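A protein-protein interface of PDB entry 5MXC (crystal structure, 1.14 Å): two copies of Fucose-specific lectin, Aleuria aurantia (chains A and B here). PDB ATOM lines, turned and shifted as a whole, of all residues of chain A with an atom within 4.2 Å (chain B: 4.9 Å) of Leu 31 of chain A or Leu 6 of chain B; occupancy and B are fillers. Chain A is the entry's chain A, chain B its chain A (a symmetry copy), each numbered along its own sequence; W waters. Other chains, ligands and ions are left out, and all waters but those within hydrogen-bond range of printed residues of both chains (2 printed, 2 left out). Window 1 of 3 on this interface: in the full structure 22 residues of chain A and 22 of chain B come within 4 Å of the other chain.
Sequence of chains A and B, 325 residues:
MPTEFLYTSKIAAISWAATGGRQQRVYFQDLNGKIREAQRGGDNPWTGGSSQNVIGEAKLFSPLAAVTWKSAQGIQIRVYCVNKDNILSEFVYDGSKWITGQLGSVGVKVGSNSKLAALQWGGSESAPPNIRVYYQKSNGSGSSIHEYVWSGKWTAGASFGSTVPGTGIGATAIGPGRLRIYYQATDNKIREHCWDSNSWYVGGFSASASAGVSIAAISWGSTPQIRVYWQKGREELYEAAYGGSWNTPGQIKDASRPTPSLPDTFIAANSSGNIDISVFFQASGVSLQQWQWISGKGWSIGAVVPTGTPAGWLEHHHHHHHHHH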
ATOM      1  N   GLU A   4      24.407  -9.609  36.092  1.00  0.00           N
ATOM      2  CA  GLU A   4      25.369 -10.358  35.285  1.00  0.00           C
ATOM      3  C   GLU A   4      25.233 -11.870  35.435  1.00  0.00           C
ATOM      4  O   GLU A   4      26.094 -12.604  34.935  1.00  0.00           O
ATOM      5  CB  GLU A   4      26.781  -9.850  35.602  1.00  0.00           C
ATOM      6  CG  GLU A   4      26.883  -8.362  35.256  1.00  0.00           C
ATOM      7  CD  GLU A   4      28.185  -7.708  35.623  1.00  0.00           C
ATOM      8  OE1 GLU A   4      28.743  -8.027  36.693  1.00  0.00           O
ATOM      9  OE2 GLU A   4      28.656  -6.849  34.829  1.00  0.00           O
ATOM     10  N   LEU A   6      24.096 -15.304  34.334  1.00  0.00           N
ATOM     11  CA  LEU A   6      23.686 -15.901  33.070  1.00  0.00           C
ATOM     12  C   LEU A   6      22.377 -16.665  33.253  1.00  0.00           C
ATOM     13  O   LEU A   6      22.286 -17.547  34.126  1.00  0.00           O
ATOM     14  CB  LEU A   6      24.787 -16.839  32.584  1.00  0.00           C
ATOM     15  CG  LEU A   6      24.542 -17.637  31.299  1.00  0.00           C
ATOM     16  CD1 LEU A   6      24.535 -16.726  30.087  1.00  0.00           C
ATOM     17  CD2 LEU A   6      25.598 -18.723  31.175  1.00  0.00           C
ATOM     18  N   ASP A  30      28.640 -16.077  34.925  1.00  0.00           N
ATOM     19  CA  ASP A  30      28.287 -14.757  34.424  1.00  0.00           C
ATOM     20  C   ASP A  30      28.160 -14.758  32.900  1.00  0.00           C
ATOM     21  O   ASP A  30      28.366 -15.777  32.230  1.00  0.00           O
ATOM     22  CB  ASP A  30      29.229 -13.676  34.989  1.00  0.00           C
ATOM     23  CG  ASP A  30      30.644 -13.722  34.431  1.00  0.00           C
ATOM     24  OD1 ASP A  30      30.883 -14.253  33.331  1.00  0.00           O
ATOM     25  OD2 ASP A  30      31.527 -13.143  35.131  1.00  0.00           O
ATOM     26  N   LEU A  31      27.824 -13.591  32.360  1.00  0.00           N
ATOM     27  CA  LEU A  31      27.578 -13.458  30.911  1.00  0.00           C
ATOM     28  C   LEU A  31      28.811 -13.710  30.076  1.00  0.00           C
ATOM     29  O   LEU A  31      28.689 -14.060  28.901  1.00  0.00           O
ATOM     30  CB  LEU A  31      27.029 -12.058  30.588  1.00  0.00           C
ATOM     31  CG  LEU A  31      25.750 -11.674  31.322  1.00  0.00           C
ATOM     32  CD1 LEU A  31      25.385 -10.239  30.990  1.00  0.00           C
ATOM     33  CD2 LEU A  31      24.611 -12.612  30.970  1.00  0.00           C
ATOM     34  N   ASN A  32      29.992 -13.543  30.687  1.00  0.00           N
ATOM     35  CA  ASN A  32      31.284 -13.781  30.036  1.00  0.00           C
ATOM     36  C   ASN A  32      31.782 -15.204  30.180  1.00  0.00           C
ATOM     37  O   ASN A  32      32.868 -15.510  29.681  1.00  0.00           O
ATOM     38  CB  ASN A  32      32.341 -12.824  30.597  1.00  0.00           C
ATOM     39  CG  ASN A  32      32.010 -11.389  30.304  1.00  0.00           C
ATOM     40  OD1 ASN A  32      31.593 -11.064  29.189  1.00  0.00           O
ATOM     41  ND2 ASN A  32      32.179 -10.533  31.281  1.00  0.00           N
ATOM     42  N   GLY A  33      31.024 -16.082  30.836  1.00  0.00           N
ATOM     43  CA  GLY A  33      31.461 -17.442  31.037  1.00  0.00           C
ATOM     44  C   GLY A  33      32.332 -17.669  32.261  1.00  0.00           C
ATOM     45  O   GLY A  33      32.751 -18.812  32.520  1.00  0.00           O
ATOM     46  N   LEU A  60      30.271 -21.674  28.217  1.00  0.00           N
ATOM     47  CA  LEU A  60      28.974 -21.075  28.540  1.00  0.00           C
ATOM     48  C   LEU A  60      27.965 -22.181  28.806  1.00  0.00           C
ATOM     49  O   LEU A  60      27.918 -23.169  28.070  1.00  0.00           O
ATOM     50  CB  LEU A  60      28.490 -20.120  27.446  1.00  0.00           C
ATOM     51  CG  LEU A  60      29.025 -18.687  27.494  1.00  0.00           C
ATOM     52  CD1 LEU A  60      28.443 -17.927  28.684  1.00  0.00           C
ATOM     53  CD2 LEU A  60      30.528 -18.586  27.475  1.00  0.00           C
ATOM     54  N   GLU B   4      23.449 -17.982  21.809  1.00  0.00           N
ATOM     55  CA  GLU B   4      24.135 -16.762  22.228  1.00  0.00           C
ATOM     56  C   GLU B   4      23.208 -15.554  22.329  1.00  0.00           C
ATOM     57  O   GLU B   4      23.699 -14.432  22.511  1.00  0.00           O
ATOM     58  CB  GLU B   4      25.331 -16.523  21.300  1.00  0.00           C
ATOM     59  CG  GLU B   4      26.300 -17.704  21.393  1.00  0.00           C
ATOM     60  CD  GLU B   4      27.466 -17.653  20.447  1.00  0.00           C
ATOM     61  OE1 GLU B   4      27.287 -17.225  19.288  1.00  0.00           O
ATOM     62  OE2 GLU B   4      28.584 -18.056  20.867  1.00  0.00           O
ATOM     63  N   PHE B   5      21.893 -15.773  22.263  1.00  0.00           N
ATOM     64  CA  PHE B   5      20.890 -14.697  22.401  1.00  0.00           C
ATOM     65  C   PHE B   5      20.775 -14.309  23.870  1.00  0.00           C
ATOM     66  O   PHE B   5      20.397 -15.138  24.700  1.00  0.00           O
ATOM     67  CB  PHE B   5      19.565 -15.256  21.870  1.00  0.00           C
ATOM     68  CG  PHE B   5      18.429 -14.270  21.673  1.00  0.00           C
ATOM     69  CD1 PHE B   5      18.548 -12.877  21.758  1.00  0.00           C
ATOM     70  CD2 PHE B   5      17.193 -14.799  21.309  1.00  0.00           C
ATOM     71  CE1 PHE B   5      17.452 -12.067  21.513  1.00  0.00           C
ATOM     72  CE2 PHE B   5      16.100 -13.984  21.078  1.00  0.00           C
ATOM     73  CZ  PHE B   5      16.238 -12.615  21.171  1.00  0.00           C
ATOM     74  N   LEU B   6      21.072 -13.056  24.198  1.00  0.00           N
ATOM     75  CA  LEU B   6      20.983 -12.603  25.580  1.00  0.00           C
ATOM     76  C   LEU B   6      19.529 -12.629  26.046  1.00  0.00           C
ATOM     77  O   LEU B   6      18.655 -12.023  25.400  1.00  0.00           O
ATOM     78  CB  LEU B   6      21.546 -11.188  25.675  1.00  0.00           C
ATOM     79  CG  LEU B   6      21.490 -10.476  27.030  1.00  0.00           C
ATOM     80  CD1 LEU B   6      22.444 -11.117  28.020  1.00  0.00           C
ATOM     81  CD2 LEU B   6      21.796  -9.000  26.835  1.00  0.00           C
ATOM     82  N   TYR B   7      19.268 -13.291  27.170  1.00  0.00           N
ATOM     83  CA  TYR B   7      17.928 -13.329  27.715  1.00  0.00           C
ATOM     84  C   TYR B   7      17.502 -11.935  28.170  1.00  0.00           C
ATOM     85  O   TYR B   7      18.225 -11.280  28.915  1.00  0.00           O
ATOM     86  CB  TYR B   7      17.859 -14.305  28.891  1.00  0.00           C
ATOM     87  CG  TYR B   7      16.541 -14.302  29.627  1.00  0.00           C
ATOM     88  CD1 TYR B   7      15.343 -14.540  28.964  1.00  0.00           C
ATOM     89  CD2 TYR B   7      16.500 -14.062  30.989  1.00  0.00           C
ATOM     90  CE1 TYR B   7      14.137 -14.525  29.643  1.00  0.00           C
ATOM     91  CE2 TYR B   7      15.305 -14.065  31.684  1.00  0.00           C
ATOM     92  CZ  TYR B   7      14.123 -14.291  31.012  1.00  0.00           C
ATOM     93  OH  TYR B   7      12.939 -14.290  31.730  1.00  0.00           O
ATOM     94  N   THR B   8      16.328 -11.498  27.719  1.00  0.00           N
ATOM     95  CA  THR B   8      15.799 -10.132  27.897  1.00  0.00           C
ATOM     96  C   THR B   8      16.526  -9.077  27.063  1.00  0.00           C
ATOM     97  O   THR B   8      16.336  -7.879  27.264  1.00  0.00           O
ATOM     98  CB  THR B   8      15.563  -9.686  29.369  1.00  0.00           C
ATOM     99  OG1 THR B   8      16.786  -9.327  30.013  1.00  0.00           O
ATOM    100  CG2 THR B   8      14.817 -10.745  30.156  1.00  0.00           C
ATOM    101  N   SER B   9      17.276  -9.519  26.053  1.00  0.00           N
ATOM    102  CA  SER B   9      17.691  -8.609  24.986  1.00  0.00           C
ATOM    103  C   SER B   9      16.478  -7.925  24.388  1.00  0.00           C
ATOM    104  O   SER B   9      15.434  -8.554  24.184  1.00  0.00           O
ATOM    105  CB  SER B   9      18.364  -9.405  23.879  1.00  0.00           C
ATOM    106  OG  SER B   9      18.730  -8.591  22.781  1.00  0.00           O
ATOM    107  N   GLN B  29      20.860  -8.637  20.820  1.00  0.00           N
ATOM    108  CA  GLN B  29      22.124  -8.581  21.529  1.00  0.00           C
ATOM    109  C   GLN B  29      22.571  -9.967  21.953  1.00  0.00           C
ATOM    110  O   GLN B  29      21.742 -10.815  22.350  1.00  0.00           O
ATOM    111  CB  GLN B  29      22.000  -7.665  22.736  1.00  0.00           C
ATOM    112  CG  GLN B  29      23.315  -7.235  23.342  1.00  0.00           C
ATOM    113  CD  GLN B  29      23.138  -6.041  24.263  1.00  0.00           C
ATOM    114  OE1 GLN B  29      22.156  -5.958  25.025  1.00  0.00           O
ATOM    115  NE2 GLN B  29      24.074  -5.103  24.208  1.00  0.00           N
ATOM    116  N   ASP B  30      23.887 -10.177  21.879  1.00  0.00           N
ATOM    117  CA  ASP B  30      24.490 -11.425  22.321  1.00  0.00           C
ATOM    118  C   ASP B  30      25.023 -11.309  23.750  1.00  0.00           C
ATOM    119  O   ASP B  30      24.944 -10.253  24.390  1.00  0.00           O
ATOM    120  CB  ASP B  30      25.516 -11.943  21.294  1.00  0.00           C
ATOM    121  CG  ASP B  30      26.798 -11.126  21.218  1.00  0.00           C
ATOM    122  OD1 ASP B  30      27.166 -10.421  22.175  1.00  0.00           O
ATOM    123  OD2 ASP B  30      27.470 -11.259  20.153  1.00  0.00           O
ATOM    124  N   LEU B  31      25.578 -12.413  24.238  1.00  0.00           N
ATOM    125  CA  LEU B  31      26.058 -12.479  25.632  1.00  0.00           C
ATOM    126  C   LEU B  31      27.211 -11.544  25.907  1.00  0.00           C
ATOM    127  O   LEU B  31      27.428 -11.167  27.059  1.00  0.00           O
ATOM    128  CB  LEU B  31      26.479 -13.915  25.985  1.00  0.00           C
ATOM    129  CG  LEU B  31      25.399 -14.974  25.805  1.00  0.00           C
ATOM    130  CD1 LEU B  31      25.982 -16.347  26.086  1.00  0.00           C
ATOM    131  CD2 LEU B  31      24.207 -14.704  26.704  1.00  0.00           C
ATOM    132  N   ASN B  32      27.940 -11.164  24.848  1.00  0.00           N
ATOM    133  CA  ASN B  32      29.069 -10.234  24.930  1.00  0.00           C
ATOM    134  C   ASN B  32      28.672  -8.782  24.761  1.00  0.00           C
ATOM    135  O   ASN B  32      29.548  -7.914  24.799  1.00  0.00           O
ATOM    136  CB  ASN B  32      30.121 -10.586  23.873  1.00  0.00           C
ATOM    137  CG  ASN B  32      30.713 -11.947  24.105  1.00  0.00           C
ATOM    138  OD1 ASN B  32      31.021 -12.303  25.245  1.00  0.00           O
ATOM    139  ND2 ASN B  32      30.869 -12.710  23.051  1.00  0.00           N
ATOM    140  N   LEU B  60      25.078  -3.772  27.924  1.00  0.00           N
ATOM    141  CA  LEU B  60      24.263  -4.977  28.097  1.00  0.00           C
ATOM    142  C   LEU B  60      22.830  -4.569  28.404  1.00  0.00           C
ATOM    143  O   LEU B  60      22.601  -3.660  29.205  1.00  0.00           O
ATOM    144  CB  LEU B  60      24.828  -5.908  29.172  1.00  0.00           C
ATOM    145  CG  LEU B  60      25.935  -6.871  28.738  1.00  0.00           C
ATOM    146  CD1 LEU B  60      25.384  -7.955  27.814  1.00  0.00           C
ATOM    147  CD2 LEU B  60      27.135  -6.198  28.122  1.00  0.00           C
ATOM    148  N   PHE B  61      21.886  -5.255  27.763  1.00  0.00           N
ATOM    149  CA  PHE B  61      20.438  -4.996  27.907  1.00  0.00           C
ATOM    150  C   PHE B  61      20.040  -3.634  27.335  1.00  0.00           C
ATOM    151  O   PHE B  61      18.990  -3.087  27.672  1.00  0.00           O
ATOM    152  CB  PHE B  61      19.944  -5.190  29.368  1.00  0.00           C
ATOM    153  CG  PHE B  61      20.421  -6.476  29.975  1.00  0.00           C
ATOM    154  CD1 PHE B  61      19.758  -7.652  29.714  1.00  0.00           C
ATOM    155  CD2 PHE B  61      21.574  -6.517  30.763  1.00  0.00           C
ATOM    156  CE1 PHE B  61      20.214  -8.850  30.245  1.00  0.00           C
ATOM    157  CE2 PHE B  61      22.033  -7.708  31.303  1.00  0.00           C
ATOM    158  CZ  PHE B  61      21.360  -8.883  31.020  1.00  0.00           C
ATOM    159  N   GLN B 282      10.943 -13.640  22.114  1.00  0.00           N
ATOM    160  CA  GLN B 282      11.996 -14.470  22.685  1.00  0.00           C
ATOM    161  C   GLN B 282      11.393 -15.581  23.535  1.00  0.00           C
ATOM    162  O   GLN B 282      10.580 -15.333  24.430  1.00  0.00           O
ATOM    163  CB  GLN B 282      12.963 -13.615  23.494  1.00  0.00           C
ATOM    164  CG  GLN B 282      14.129 -14.387  24.090  1.00  0.00           C
ATOM    165  CD  GLN B 282      15.110 -13.471  24.796  1.00  0.00           C
ATOM    166  OE1 GLN B 282      14.748 -12.810  25.764  1.00  0.00           O
ATOM    167  NE2 GLN B 282      16.347 -13.434  24.338  1.00  0.00           N
HETATM  168  O   HOH W   1      29.292  -9.765  28.522  1.00  0.00           O
HETATM  169  O   HOH W   2      30.205 -14.495  26.645  1.00  0.00           O
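Of the 13 printed residues of chain B, 3 touch a printed residue of chain A.
Hydrophobic or aromatic side chains of chain B within 4 Å of the printed part of chain A: Leu 6, Leu 31 and Leu 60.
Of the 7 printed residues of chain A, 3 touch a printed residue of chain B.
Printed residues of chain A that touch a printed residue of chain B: Leu 6, Leu 31 and Leu 60.
Among the printed residues, 5 pairs touch across the chains.
Among the printed residues, no Asp or Glu carboxylate lies within 4 Å of a Lys or Arg side-chain nitrogen of the other chain.
Of chain B, only Leu 6 (3.95 Å), Leu 31 (3.7 Å) and Leu 60 (3.9 Å) come within 4 Å of Leu 31 of chain A.
Gly 33 of chain A touches none of the printed residues of chain B.
Printed residues of chain B within 4 Å of Leu 60 of chain A: Leu 31.
Printed residues of chain A within 4 Å of Leu 6 of chain B: Leu 31.
Printed residues of chain A within 4 Å of Leu 31 of chain B: Leu 6, Leu 31 and Leu 60.
Of the printed residues of chain A, Leu 60 of chain B touches Leu 31.
The nearest printed residue of chain A that does not touch Leu 6 of chain B is Leu 6 of chain A (6.3 Å).
The nearest printed residue of chain A that does not touch Leu 31 of chain B is Asn 32 of chain A (4.7 Å).
Leu 6 of chain A touches Leu 31 of chain B, and with the chains exchanged Leu 31 of chain A touches Leu 6 of chain B.
Leu 31 of chain A touches its own counterpart, Leu 31 of chain B.
Leu 31 of chain A touches Leu 60 of chain B, and with the chains exchanged Leu 60 of chain A touches Leu 31 of chain B.
Positions printed for both chains: 4, 6, 30, 31, 32 and 60.
Of the 5 pairs that touch across the chains among the printed residues, 5 have their exchanged pair printed and touching as well.
The backbone NH of Leu 6 of chain B sits at hydrogen-bond distance from the backbone carbonyl oxygen of Gln 29 of chain B (3.0 Å).
The backbone carbonyl oxygen of Leu 6 of chain B lies within hydrogen-bond range of the side-chain amide nitrogen of Gln 282 of chain B (2.9 Å).
The backbone carbonyl oxygen (O) of Glu 4 of chain A is in hydrogen-bond range of the backbone NH (N) of Leu 31 of chain A (3.3 Å).
The backbone NH (N) of Leu 31 of chain B sits at hydrogen-bond distance from the backbone carbonyl oxygen (O) of Glu 4 of chain B, 3.3 Å away.
Among the printed residues, pairs that only touch across the chains: Leu 6 of chain A with Leu 31 of chain B (3.95 Å), Leu 31 of chain A with Leu 6 of chain B (3.95 Å), Leu 31 of chain A with Leu 31 of chain B (3.7 Å), Leu 31 of chain A with Leu 60 of chain B (3.9 Å) and Leu 60 of chain A with Leu 31 of chain B (3.9 Å).
Water W1 bridges the side-chain amide oxygen (OD1) of Asn 32 of chain A (2.7 Å) and the backbone carbonyl oxygen (O) of Leu 31 of chain B (2.8 Å).
Water W2 lies within hydrogen-bond range of the side-chain amide oxygen (OD1) of Asn 32 of chain B (2.7 Å) and the backbone carbonyl oxygen (O) of Leu 31 of chain A (2.8 Å).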
